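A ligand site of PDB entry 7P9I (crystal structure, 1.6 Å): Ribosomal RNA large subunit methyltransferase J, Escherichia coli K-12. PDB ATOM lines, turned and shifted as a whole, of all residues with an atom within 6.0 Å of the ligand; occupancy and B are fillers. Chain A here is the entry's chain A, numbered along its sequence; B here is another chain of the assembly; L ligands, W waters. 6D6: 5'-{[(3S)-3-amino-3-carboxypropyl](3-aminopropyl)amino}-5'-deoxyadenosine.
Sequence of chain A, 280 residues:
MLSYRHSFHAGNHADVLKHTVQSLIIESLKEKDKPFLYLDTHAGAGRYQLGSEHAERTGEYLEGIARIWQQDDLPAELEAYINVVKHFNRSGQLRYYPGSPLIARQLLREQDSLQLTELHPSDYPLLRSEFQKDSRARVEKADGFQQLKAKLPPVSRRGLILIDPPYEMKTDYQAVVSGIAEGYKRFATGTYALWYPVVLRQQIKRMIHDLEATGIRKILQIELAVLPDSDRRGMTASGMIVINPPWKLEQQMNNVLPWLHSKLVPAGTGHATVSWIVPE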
ATOM      1  N   ARG A   5      -4.324  37.089   9.093  1.00  0.00           N
ATOM      2  CA  ARG A   5      -4.126  36.946  10.527  1.00  0.00           C
ATOM      3  C   ARG A   5      -3.174  38.018  11.052  1.00  0.00           C
ATOM      4  O   ARG A   5      -2.098  38.255  10.496  1.00  0.00           O
ATOM      5  CB  ARG A   5      -3.571  35.546  10.836  1.00  0.00           C
ATOM      6  CG  ARG A   5      -3.239  35.339  12.312  1.00  0.00           C
ATOM      7  CD  ARG A   5      -4.528  35.299  13.125  1.00  0.00           C
ATOM      8  NE  ARG A   5      -5.422  34.249  12.616  1.00  0.00           N
ATOM      9  CZ  ARG A   5      -6.634  34.461  12.103  1.00  0.00           C
ATOM     10  NH1 ARG A   5      -7.155  35.684  12.052  1.00  0.00           N
ATOM     11  NH2 ARG A   5      -7.333  33.415  11.652  1.00  0.00           N
ATOM     12  N   SER A   7      -0.702  39.277  14.206  1.00  0.00           N
ATOM     13  CA  SER A   7       0.154  38.565  15.160  1.00  0.00           C
ATOM     14  C   SER A   7       1.146  39.516  15.800  1.00  0.00           C
ATOM     15  O   SER A   7       2.036  40.041  15.120  1.00  0.00           O
ATOM     16  CB  SER A   7       0.884  37.416  14.475  1.00  0.00           C
ATOM     17  OG  SER A   7       2.116  37.214  15.140  1.00  0.00           O
ATOM     18  N   ASP A  15      11.716  35.348  14.244  1.00  0.00           N
ATOM     19  CA  ASP A  15      11.318  35.144  12.858  1.00  0.00           C
ATOM     20  C   ASP A  15      12.450  35.543  11.911  1.00  0.00           C
ATOM     21  O   ASP A  15      12.720  34.851  10.912  1.00  0.00           O
ATOM     22  CB  ASP A  15      10.053  35.948  12.547  1.00  0.00           C
ATOM     23  CG  ASP A  15       8.793  35.286  13.073  1.00  0.00           C
ATOM     24  OD1 ASP A  15       8.857  34.106  13.497  1.00  0.00           O
ATOM     25  OD2 ASP A  15       7.736  35.957  13.063  1.00  0.00           O
ATOM     26  N   LYS A  18      14.973  32.683  12.018  1.00  0.00           N
ATOM     27  CA  LYS A  18      14.386  31.457  11.421  1.00  0.00           C
ATOM     28  C   LYS A  18      14.303  31.590   9.901  1.00  0.00           C
ATOM     29  O   LYS A  18      14.616  30.665   9.273  1.00  0.00           O
ATOM     30  CB  LYS A  18      12.978  31.224  11.978  1.00  0.00           C
ATOM     31  CG  LYS A  18      12.192  30.034  11.394  1.00  0.00           C
ATOM     32  CD  LYS A  18      10.767  29.918  12.017  1.00  0.00           C
ATOM     33  CE  LYS A  18      10.057  31.287  12.090  1.00  0.00           C
ATOM     34  NZ  LYS A  18       8.586  31.158  12.336  1.00  0.00           N
ATOM     35  N   HIS A  19      13.789  32.699   9.365  1.00  0.00           N
ATOM     36  CA  HIS A  19      13.591  32.842   7.931  1.00  0.00           C
ATOM     37  C   HIS A  19      14.876  33.165   7.204  1.00  0.00           C
ATOM     38  O   HIS A  19      15.015  32.832   6.025  1.00  0.00           O
ATOM     39  CB  HIS A  19      12.505  33.884   7.679  1.00  0.00           C
ATOM     40  CG  HIS A  19      11.155  33.445   8.188  1.00  0.00           C
ATOM     41  ND1 HIS A  19      10.248  34.314   8.754  1.00  0.00           N
ATOM     42  CD2 HIS A  19      10.601  32.218   8.244  1.00  0.00           C
ATOM     43  CE1 HIS A  19       9.169  33.630   9.121  1.00  0.00           C
ATOM     44  NE2 HIS A  19       9.357  32.354   8.815  1.00  0.00           N
ATOM     45  N   GLN A  22      16.251  29.591   6.927  1.00  0.00           N
ATOM     46  CA  GLN A  22      15.444  28.928   5.909  1.00  0.00           C
ATOM     47  C   GLN A  22      15.849  29.361   4.500  1.00  0.00           C
ATOM     48  O   GLN A  22      16.047  28.514   3.618  1.00  0.00           O
ATOM     49  CB  GLN A  22      13.952  29.223   6.136  1.00  0.00           C
ATOM     50  CG  GLN A  22      13.008  28.521   5.104  1.00  0.00           C
ATOM     51  CD  GLN A  22      11.596  29.097   5.109  1.00  0.00           C
ATOM     52  OE1 GLN A  22      11.243  29.894   5.971  1.00  0.00           O
ATOM     53  NE2 GLN A  22      10.779  28.685   4.138  1.00  0.00           N
ATOM     54  N   ASP A  40       6.962  21.696   5.422  1.00  0.00           N
ATOM     55  CA  ASP A  40       6.716  22.623   6.533  1.00  0.00           C
ATOM     56  C   ASP A  40       5.710  21.958   7.461  1.00  0.00           C
ATOM     57  O   ASP A  40       4.508  21.925   7.164  1.00  0.00           O
ATOM     58  CB  ASP A  40       6.209  23.942   5.964  1.00  0.00           C
ATOM     59  CG  ASP A  40       6.380  25.120   6.920  1.00  0.00           C
ATOM     60  OD1 ASP A  40       6.262  24.950   8.143  1.00  0.00           O
ATOM     61  OD2 ASP A  40       6.586  26.241   6.408  1.00  0.00           O
ATOM     62  N   HIS A  42       4.677  22.630  10.610  1.00  0.00           N
ATOM     63  CA  HIS A  42       3.825  23.574  11.391  1.00  0.00           C
ATOM     64  C   HIS A  42       3.841  24.857  10.568  1.00  0.00           C
ATOM     65  O   HIS A  42       4.660  25.671  10.840  1.00  0.00           O
ATOM     66  CB  HIS A  42       4.344  23.692  12.833  1.00  0.00           C
ATOM     67  CG  HIS A  42       4.376  22.404  13.560  1.00  0.00           C
ATOM     68  ND1 HIS A  42       3.258  21.740  13.998  1.00  0.00           N
ATOM     69  CD2 HIS A  42       5.410  21.623  13.895  1.00  0.00           C
ATOM     70  CE1 HIS A  42       3.626  20.599  14.551  1.00  0.00           C
ATOM     71  NE2 HIS A  42       4.932  20.497  14.480  1.00  0.00           N
ATOM     72  N   ALA A  43       2.974  24.981   9.577  1.00  0.00           N
ATOM     73  CA  ALA A  43       3.133  26.011   8.565  1.00  0.00           C
ATOM     74  C   ALA A  43       2.447  27.325   8.900  1.00  0.00           C
ATOM     75  O   ALA A  43       2.789  28.352   8.298  1.00  0.00           O
ATOM     76  CB  ALA A  43       2.610  25.471   7.211  1.00  0.00           C
ATOM     77  N   GLY A  44       1.507  27.344   9.846  1.00  0.00           N
ATOM     78  CA  GLY A  44       0.848  28.608  10.216  1.00  0.00           C
ATOM     79  C   GLY A  44      -0.103  29.123   9.156  1.00  0.00           C
ATOM     80  O   GLY A  44      -0.573  28.396   8.270  1.00  0.00           O
ATOM     81  N   ALA A  45      -0.384  30.437   9.255  1.00  0.00           N
ATOM     82  CA  ALA A  45      -1.368  31.073   8.383  1.00  0.00           C
ATOM     83  C   ALA A  45      -0.816  31.382   6.993  1.00  0.00           C
ATOM     84  O   ALA A  45      -1.595  31.482   6.034  1.00  0.00           O
ATOM     85  CB  ALA A  45      -1.884  32.352   9.035  1.00  0.00           C
ATOM     86  N   GLY A  46       0.507  31.567   6.858  1.00  0.00           N
ATOM     87  CA  GLY A  46       1.129  31.870   5.584  1.00  0.00           C
ATOM     88  C   GLY A  46       1.740  33.257   5.524  1.00  0.00           C
ATOM     89  O   GLY A  46       2.841  33.441   5.012  1.00  0.00           O
ATOM     90  N   TYR A  48       1.269  37.372   7.790  1.00  0.00           N
ATOM     91  CA  TYR A  48       0.773  38.012   8.996  1.00  0.00           C
ATOM     92  C   TYR A  48       0.655  39.495   8.716  1.00  0.00           C
ATOM     93  O   TYR A  48       1.574  40.104   8.165  1.00  0.00           O
ATOM     94  CB  TYR A  48       1.701  37.712  10.197  1.00  0.00           C
ATOM     95  CG  TYR A  48       1.670  36.231  10.470  1.00  0.00           C
ATOM     96  CD1 TYR A  48       0.656  35.677  11.224  1.00  0.00           C
ATOM     97  CD2 TYR A  48       2.600  35.380   9.881  1.00  0.00           C
ATOM     98  CE1 TYR A  48       0.576  34.305  11.430  1.00  0.00           C
ATOM     99  CE2 TYR A  48       2.532  34.008  10.068  1.00  0.00           C
ATOM    100  CZ  TYR A  48       1.524  33.466  10.848  1.00  0.00           C
ATOM    101  OH  TYR A  48       1.437  32.101  11.043  1.00  0.00           O
ATOM    102  N   PRO A  98       5.870  37.895   5.605  1.00  0.00           N
ATOM    103  CA  PRO A  98       5.656  36.555   5.021  1.00  0.00           C
ATOM    104  C   PRO A  98       6.118  35.477   5.972  1.00  0.00           C
ATOM    105  O   PRO A  98       7.222  35.543   6.509  1.00  0.00           O
ATOM    106  CB  PRO A  98       6.514  36.584   3.748  1.00  0.00           C
ATOM    107  CG  PRO A  98       7.640  37.538   4.090  1.00  0.00           C
ATOM    108  CD  PRO A  98       7.062  38.577   5.061  1.00  0.00           C
ATOM    109  N   GLY A  99       5.289  34.445   6.148  1.00  0.00           N
ATOM    110  CA  GLY A  99       5.669  33.288   6.940  1.00  0.00           C
ATOM    111  C   GLY A  99       6.531  32.319   6.143  1.00  0.00           C
ATOM    112  O   GLY A  99       6.757  32.479   4.950  1.00  0.00           O
ATOM    113  N   SER A 100       6.996  31.280   6.833  1.00  0.00           N
ATOM    114  CA  SER A 100       7.836  30.284   6.152  1.00  0.00           C
ATOM    115  C   SER A 100       7.199  29.733   4.879  1.00  0.00           C
ATOM    116  O   SER A 100       7.928  29.504   3.908  1.00  0.00           O
ATOM    117  CB  SER A 100       8.201  29.161   7.147  1.00  0.00           C
ATOM    118  OG  SER A 100       7.060  28.481   7.639  1.00  0.00           O
ATOM    119  N   PRO A 101       5.878  29.491   4.792  1.00  0.00           N
ATOM    120  CA  PRO A 101       5.325  28.987   3.525  1.00  0.00           C
ATOM    121  C   PRO A 101       5.493  29.958   2.354  1.00  0.00           C
ATOM    122  O   PRO A 101       5.713  29.508   1.214  1.00  0.00           O
ATOM    123  CB  PRO A 101       3.836  28.733   3.853  1.00  0.00           C
ATOM    124  CG  PRO A 101       3.771  28.659   5.338  1.00  0.00           C
ATOM    125  CD  PRO A 101       4.840  29.590   5.842  1.00  0.00           C
ATOM    126  N   GLU A 118      -1.002  22.359   8.745  1.00  0.00           N
ATOM    127  CA  GLU A 118      -1.365  23.239   9.833  1.00  0.00           C
ATOM    128  C   GLU A 118      -2.713  22.788  10.372  1.00  0.00           C
ATOM    129  O   GLU A 118      -3.656  22.635   9.584  1.00  0.00           O
ATOM    130  CB  GLU A 118      -1.441  24.699   9.379  1.00  0.00           C
ATOM    131  CG  GLU A 118      -1.863  25.660  10.465  1.00  0.00           C
ATOM    132  CD  GLU A 118      -1.054  25.482  11.745  1.00  0.00           C
ATOM    133  OE1 GLU A 118       0.190  25.618  11.709  1.00  0.00           O
ATOM    134  OE2 GLU A 118      -1.660  25.187  12.794  1.00  0.00           O
ATOM    135  N   HIS A 120      -4.392  24.511  12.914  1.00  0.00           N
ATOM    136  CA  HIS A 120      -5.156  25.629  13.461  1.00  0.00           C
ATOM    137  C   HIS A 120      -6.424  25.832  12.643  1.00  0.00           C
ATOM    138  O   HIS A 120      -6.355  25.997  11.410  1.00  0.00           O
ATOM    139  CB  HIS A 120      -4.284  26.873  13.468  1.00  0.00           C
ATOM    140  CG  HIS A 120      -4.812  28.005  14.293  1.00  0.00           C
ATOM    141  ND1 HIS A 120      -5.891  28.766  13.913  1.00  0.00           N
ATOM    142  CD2 HIS A 120      -4.368  28.532  15.461  1.00  0.00           C
ATOM    143  CE1 HIS A 120      -6.104  29.710  14.815  1.00  0.00           C
ATOM    144  NE2 HIS A 120      -5.195  29.575  15.769  1.00  0.00           N
ATOM    145  N   ASP A 123      -6.387  29.325  10.891  1.00  0.00           N
ATOM    146  CA  ASP A 123      -5.267  29.651  10.040  1.00  0.00           C
ATOM    147  C   ASP A 123      -5.083  28.673   8.895  1.00  0.00           C
ATOM    148  O   ASP A 123      -4.503  29.046   7.870  1.00  0.00           O
ATOM    149  CB  ASP A 123      -3.975  29.751  10.871  1.00  0.00           C
ATOM    150  CG  ASP A 123      -3.988  30.951  11.819  1.00  0.00           C
ATOM    151  OD1 ASP A 123      -4.928  31.781  11.743  1.00  0.00           O
ATOM    152  OD2 ASP A 123      -3.044  31.068  12.640  1.00  0.00           O
ATOM    153  N   LEU A 162      11.326  21.891   7.543  1.00  0.00           N
ATOM    154  CA  LEU A 162      11.299  22.912   8.582  1.00  0.00           C
ATOM    155  C   LEU A 162      10.287  22.512   9.655  1.00  0.00           C
ATOM    156  O   LEU A 162       9.135  22.241   9.343  1.00  0.00           O
ATOM    157  CB  LEU A 162      10.924  24.279   8.007  1.00  0.00           C
ATOM    158  CG  LEU A 162      10.661  25.279   9.143  1.00  0.00           C
ATOM    159  CD1 LEU A 162      11.973  25.683   9.819  1.00  0.00           C
ATOM    160  CD2 LEU A 162       9.910  26.481   8.647  1.00  0.00           C
ATOM    161  N   ASP A 164       8.674  23.856  13.134  1.00  0.00           N
ATOM    162  CA  ASP A 164       8.527  25.154  13.797  1.00  0.00           C
ATOM    163  C   ASP A 164       7.289  25.092  14.698  1.00  0.00           C
ATOM    164  O   ASP A 164       6.266  25.737  14.427  1.00  0.00           O
ATOM    165  CB  ASP A 164       8.429  26.257  12.743  1.00  0.00           C
ATOM    166  CG  ASP A 164       8.399  27.652  13.316  1.00  0.00           C
ATOM    167  OD1 ASP A 164       8.823  27.858  14.478  1.00  0.00           O
ATOM    168  OD2 ASP A 164       7.929  28.535  12.568  1.00  0.00           O
ATOM    169  N   PRO A 165       7.363  24.336  15.788  1.00  0.00           N
ATOM    170  CA  PRO A 165       6.135  23.970  16.515  1.00  0.00           C
ATOM    171  C   PRO A 165       5.913  24.829  17.751  1.00  0.00           C
ATOM    172  O   PRO A 165       6.824  25.504  18.248  1.00  0.00           O
ATOM    173  CB  PRO A 165       6.416  22.522  16.917  1.00  0.00           C
ATOM    174  CG  PRO A 165       7.930  22.537  17.216  1.00  0.00           C
ATOM    175  CD  PRO A 165       8.535  23.589  16.293  1.00  0.00           C
ATOM    176  N   PRO A 166       4.695  24.789  18.305  1.00  0.00           N
ATOM    177  CA  PRO A 166       4.484  25.373  19.635  1.00  0.00           C
ATOM    178  C   PRO A 166       5.171  24.538  20.696  1.00  0.00           C
ATOM    179  O   PRO A 166       5.126  23.306  20.680  1.00  0.00           O
ATOM    180  CB  PRO A 166       2.952  25.330  19.796  1.00  0.00           C
ATOM    181  CG  PRO A 166       2.395  24.953  18.443  1.00  0.00           C
ATOM    182  CD  PRO A 166       3.482  24.166  17.763  1.00  0.00           C
ATOM    183  N   TYR A 167       5.822  25.222  21.627  1.00  0.00           N
ATOM    184  CA  TYR A 167       6.424  24.589  22.793  1.00  0.00           C
ATOM    185  C   TYR A 167       5.626  25.045  24.013  1.00  0.00           C
ATOM    186  O   TYR A 167       5.853  26.138  24.532  1.00  0.00           O
ATOM    187  CB  TYR A 167       7.898  24.943  22.934  1.00  0.00           C
ATOM    188  CG  TYR A 167       8.816  24.448  21.842  1.00  0.00           C
ATOM    189  CD1 TYR A 167       9.000  25.184  20.671  1.00  0.00           C
ATOM    190  CD2 TYR A 167       9.545  23.278  21.997  1.00  0.00           C
ATOM    191  CE1 TYR A 167       9.873  24.741  19.677  1.00  0.00           C
ATOM    192  CE2 TYR A 167      10.421  22.841  21.016  1.00  0.00           C
ATOM    193  CZ  TYR A 167      10.585  23.582  19.863  1.00  0.00           C
ATOM    194  OH  TYR A 167      11.457  23.158  18.883  1.00  0.00           O
ATOM    195  N   GLU A 168       4.701  24.214  24.458  1.00  0.00           N
ATOM    196  CA  GLU A 168       3.725  24.640  25.461  1.00  0.00           C
ATOM    197  C   GLU A 168       3.826  23.891  26.766  1.00  0.00           C
ATOM    198  O   GLU A 168       3.213  24.324  27.755  1.00  0.00           O
ATOM    199  CB  GLU A 168       2.316  24.500  24.901  1.00  0.00           C
ATOM    200  CG  GLU A 168       2.154  25.306  23.629  1.00  0.00           C
ATOM    201  CD  GLU A 168       0.736  25.771  23.409  1.00  0.00           C
ATOM    202  OE1 GLU A 168      -0.155  24.901  23.454  1.00  0.00           O
ATOM    203  OE2 GLU A 168       0.526  26.977  23.182  1.00  0.00           O
ATOM    204  N   TRP A 195      13.289  25.065  14.737  1.00  0.00           N
ATOM    205  CA  TRP A 195      13.328  26.297  15.503  1.00  0.00           C
ATOM    206  C   TRP A 195      12.974  25.998  16.964  1.00  0.00           C
ATOM    207  O   TRP A 195      12.087  25.178  17.241  1.00  0.00           O
ATOM    208  CB  TRP A 195      12.351  27.317  14.932  1.00  0.00           C
ATOM    209  CG  TRP A 195      12.376  28.608  15.720  1.00  0.00           C
ATOM    210  CD1 TRP A 195      13.239  29.661  15.566  1.00  0.00           C
ATOM    211  CD2 TRP A 195      11.519  28.948  16.819  1.00  0.00           C
ATOM    212  NE1 TRP A 195      12.963  30.639  16.506  1.00  0.00           N
ATOM    213  CE2 TRP A 195      11.903  30.229  17.265  1.00  0.00           C
ATOM    214  CE3 TRP A 195      10.456  28.297  17.447  1.00  0.00           C
ATOM    215  CZ2 TRP A 195      11.270  30.858  18.338  1.00  0.00           C
ATOM    216  CZ3 TRP A 195       9.827  28.931  18.501  1.00  0.00           C
ATOM    217  CH2 TRP A 195      10.228  30.198  18.926  1.00  0.00           C
ATOM    218  O5' GMP B   1       2.291  30.536  21.301  1.00  0.00           O
ATOM    219  C5' GMP B   1       3.200  31.575  21.006  1.00  0.00           C
ATOM    220  C4' GMP B   1       2.533  32.643  20.317  1.00  0.00           C
ATOM    221  O4' GMP B   1       1.805  32.138  19.090  1.00  0.00           O
ATOM    222  C3' GMP B   1       1.415  33.267  21.140  1.00  0.00           C
ATOM    223  O3' GMP B   1       1.950  34.278  21.928  1.00  0.00           O
ATOM    224  C2' GMP B   1       0.590  33.718  20.276  1.00  0.00           C
ATOM    225  O2' GMP B   1       0.776  35.094  20.060  1.00  0.00           O
ATOM    226  C1' GMP B   1       0.879  32.960  18.878  1.00  0.00           C
ATOM    227  N9  GMP B   1      -0.318  32.213  18.425  1.00  0.00           N
ATOM    228  C8  GMP B   1      -0.860  32.241  17.223  1.00  0.00           C
ATOM    229  N7  GMP B   1      -1.900  31.424  17.180  1.00  0.00           N
ATOM    230  C5  GMP B   1      -2.029  30.869  18.393  1.00  0.00           C
ATOM    231  C6  GMP B   1      -3.014  29.866  18.985  1.00  0.00           C
ATOM    232  O6  GMP B   1      -3.893  29.416  18.337  1.00  0.00           O
ATOM    233  N1  GMP B   1      -2.861  29.455  20.337  1.00  0.00           N
ATOM    234  C2  GMP B   1      -1.790  29.995  21.146  1.00  0.00           C
ATOM    235  N2  GMP B   1      -1.632  29.595  22.524  1.00  0.00           N
ATOM    236  N3  GMP B   1      -0.855  30.955  20.587  1.00  0.00           N
ATOM    237  C4  GMP B   1      -1.011  31.374  19.184  1.00  0.00           C
ATOM    238  P     A B   2       1.986  34.115  23.578  1.00  0.00           P
ATOM    239  OP1   A B   2       0.689  33.569  24.103  1.00  0.00           O
ATOM    240  OP2   A B   2       2.286  35.443  24.165  1.00  0.00           O
ATOM    241  O5'   A B   2       3.233  33.113  24.047  1.00  0.00           O
ATOM    242  C5'   A B   2       4.534  33.617  23.847  1.00  0.00           C
ATOM    243  C4'   A B   2       5.443  32.769  24.519  1.00  0.00           C
ATOM    244  O4'   A B   2       5.316  31.349  24.026  1.00  0.00           O
ATOM    245  C3'   A B   2       6.859  33.177  24.171  1.00  0.00           C
ATOM    246  O3'   A B   2       7.311  34.048  25.223  1.00  0.00           O
ATOM    247  C2'   A B   2       7.525  32.090  24.041  1.00  0.00           C
ATOM    248  O2'   A B   2       8.360  31.861  25.148  1.00  0.00           O
ATOM    249  C1'   A B   2       6.485  30.869  23.997  1.00  0.00           C
ATOM    250  N9    A B   2       6.541  30.042  22.759  1.00  0.00           N
ATOM    251  C8    A B   2       6.536  28.739  22.744  1.00  0.00           C
ATOM    252  N7    A B   2       6.563  28.303  21.488  1.00  0.00           N
ATOM    253  C5    A B   2       6.572  29.372  20.675  1.00  0.00           C
ATOM    254  C6    A B   2       6.588  29.551  19.279  1.00  0.00           C
ATOM    255  N6    A B   2       6.610  28.334  18.402  1.00  0.00           N
ATOM    256  N1    A B   2       6.591  30.780  18.775  1.00  0.00           N
ATOM    257  C2    A B   2       6.573  31.836  19.594  1.00  0.00           C
ATOM    258  N3    A B   2       6.561  31.718  20.911  1.00  0.00           N
ATOM    259  C4    A B   2       6.552  30.505  21.481  1.00  0.00           C
HETATM  260  C1  6D6 L   1       6.638  28.485  16.929  1.00  0.00           C
HETATM  261  C2  6D6 L   1       5.209  28.878  16.376  1.00  0.00           C
HETATM  262  C3  6D6 L   1       5.268  29.072  14.793  1.00  0.00           C
HETATM  263  C4  6D6 L   1       4.229  28.405  12.686  1.00  0.00           C
HETATM  264  C5  6D6 L   1       5.308  29.257  10.489  1.00  0.00           C
HETATM  265  C6  6D6 L   1       3.022  29.876  14.287  1.00  0.00           C
HETATM  266  C7  6D6 L   1       0.626  30.403  14.283  1.00  0.00           C
HETATM  267  C8  6D6 L   1      -1.111  26.732  15.955  1.00  0.00           C
HETATM  268  C9  6D6 L   1      -0.265  27.424  17.843  1.00  0.00           C
HETATM  269  N2  6D6 L   1       3.961  28.761  14.149  1.00  0.00           N
HETATM  270  C10 6D6 L   1       4.894  29.618  11.926  1.00  0.00           C
HETATM  271  N3  6D6 L   1       6.215  28.139  10.481  1.00  0.00           N
HETATM  272  C11 6D6 L   1       6.002  30.478   9.904  1.00  0.00           C
HETATM  273  O1  6D6 L   1       5.350  31.484   9.547  1.00  0.00           O
HETATM  274  O2  6D6 L   1       7.242  30.460   9.799  1.00  0.00           O
HETATM  275  C12 6D6 L   1       1.778  29.561  13.728  1.00  0.00           C
HETATM  276  O3  6D6 L   1       1.358  28.096  14.129  1.00  0.00           O
HETATM  277  C13 6D6 L   1       0.093  28.097  14.288  1.00  0.00           C
HETATM  278  C14 6D6 L   1      -0.424  29.653  14.055  1.00  0.00           C
HETATM  279  O4  6D6 L   1      -0.869  29.738  12.738  1.00  0.00           O
HETATM  280  O5  6D6 L   1       0.539  31.620  13.612  1.00  0.00           O
HETATM  281  N4  6D6 L   1      -0.230  27.660  15.649  1.00  0.00           N
HETATM  282  N5  6D6 L   1      -1.145  26.576  17.280  1.00  0.00           N
HETATM  283  C15 6D6 L   1       0.167  27.741  19.158  1.00  0.00           C
HETATM  284  N6  6D6 L   1      -0.412  27.059  20.320  1.00  0.00           N
HETATM  285  N7  6D6 L   1       1.093  28.654  19.349  1.00  0.00           N
HETATM  286  C16 6D6 L   1       1.624  29.284  18.312  1.00  0.00           C
HETATM  287  N8  6D6 L   1       1.257  29.027  17.065  1.00  0.00           N
HETATM  288  C17 6D6 L   1       0.324  28.116  16.811  1.00  0.00           C
HETATM  289  O   HOH W   1       6.264  34.006  10.531  1.00  0.00           O
HETATM  290  O   HOH W   2       2.837  31.031   8.403  1.00  0.00           O
HETATM  291  O   HOH W   3       1.402  24.958  14.069  1.00  0.00           O
HETATM  292  O   HOH W   4      -2.511  25.772  22.087  1.00  0.00           O
HETATM  293  O   HOH W   5       3.575  26.126  14.993  1.00  0.00           O
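C1 of the ligand is covalently linked to N6 of A 2 of chain B. The side-chain carboxylate of Asp 123 lies within hydrogen-bond range of an oxygen (O4) of the ligand (2.6 Å). OD2 of Asp 164 is in salt-bridge range of N3 of the ligand (2.7 Å). O5 of the ligand lies within hydrogen-bond range of OH of Tyr 48, at 2.8 Å. An oxygen (O2) of the ligand lies within hydrogen-bond range of the backbone NH of Ser 100, 3.1 Å away. OG of Ser 100 lies within hydrogen-bond range of O2 of the ligand (2.9 Å). The backbone carbonyl oxygen (O) of His 42 lies within hydrogen-bond range of a nitrogen (N3) of the ligand, 2.9 Å away. An oxygen (O2) of the ligand lies within salt-bridge range of the side-chain amino group (NZ) of Lys 18, 3.0 Å away. O5' of GMP 1 of chain B sits at hydrogen-bond distance from a nitrogen (N7) of the ligand, 3.0 Å away. O2 of the ligand lies within hydrogen-bond range of NE2 of His 19, 3.0 Å away. A nitrogen (N6) of the ligand is in hydrogen-bond range of the side-chain carboxylate (OE2) of Glu 168 (3.0 Å). The side-chain carboxylate of Asp 40 lies within salt-bridge range of a nitrogen (N3) of the ligand (3.95 Å).
N7 of A 2 of chain B sits at hydrogen-bond distance from N of Tyr 167 (3.2 Å). OH of Tyr 48 is in hydrogen-bond range of N of Ala 45, at 3.0 Å. The side-chain carboxylate (OD2) of Asp 40 sits at hydrogen-bond distance from the side-chain hydroxyl (OG) of Ser 100 (2.6 Å). N2 of GMP 1 of chain B is in hydrogen-bond range of OE2 of Glu 168, at 3.5 Å. NE2 of His 120 is in hydrogen-bond range of O6 of GMP 1 of chain B (2.9 Å). The backbone carbonyl oxygen (O) of Asp 15 sits at hydrogen-bond distance from a ring nitrogen (ND1) of His 19 (3.3 Å). The backbone NH (N) of Gly 99 is in hydrogen-bond range of the backbone carbonyl oxygen (O) of Gly 46 (2.9 Å). OE2 of Glu 118 is in hydrogen-bond range of N of His 120 (2.8 Å).
Ala 43 touches the ligand. Gly 44 touches the ligand. Ala 45 touches the ligand (N to O4, 3.6 Å). Gly 99 touches the ligand (CA to O1, 3.2 Å). Glu 118 touches the ligand. His 120 touches the ligand. O of Pro 165 touches C1 of the ligand, at 3.3 Å. Pro 166 touches the ligand (CG to C15, 3.6 Å). Trp 195 touches the ligand. Hydrophobic or aromatic side chains that line the ligand: His 19, Tyr 48, His 120, Pro 166 and Trp 195. Within 4 Å of the ligand: Lys 18, His 19, Asp 40, His 42, Ala 43, Gly 44, Ala 45, Tyr 48, Gly 99, Ser 100, Glu 118, His 120, Asp 123, Asp 164, Pro 165, Pro 166, Glu 168, Trp 195, GMP 1 of chain B and A 2 of chain B. Along chain A the residues within 4 Å of the ligand span positions 18 to 195. The nearest printed residue that does not touch the ligand is Pro 101 (4.2 Å).
Water W5 bridges O of Asp 164 and O3 of the ligand. Water W2 lies within hydrogen-bond range of the backbone carbonyl oxygen of Ala 43 (2.7 Å), an oxygen (O1) of the ligand (2.8 Å), the backbone NH of Gly 46 (2.8 Å), the side-chain hydroxyl of Tyr 48 (3.2 Å) and the backbone NH of Ala 45 (3.4 Å). Water W4 lies within hydrogen-bond range of the side-chain carboxylate of Glu 168 (2.9 Å) and a nitrogen (N6) of the ligand (3.0 Å). Water W3 lies within hydrogen-bond range of OE1 of Glu 118 and O3 of the ligand.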
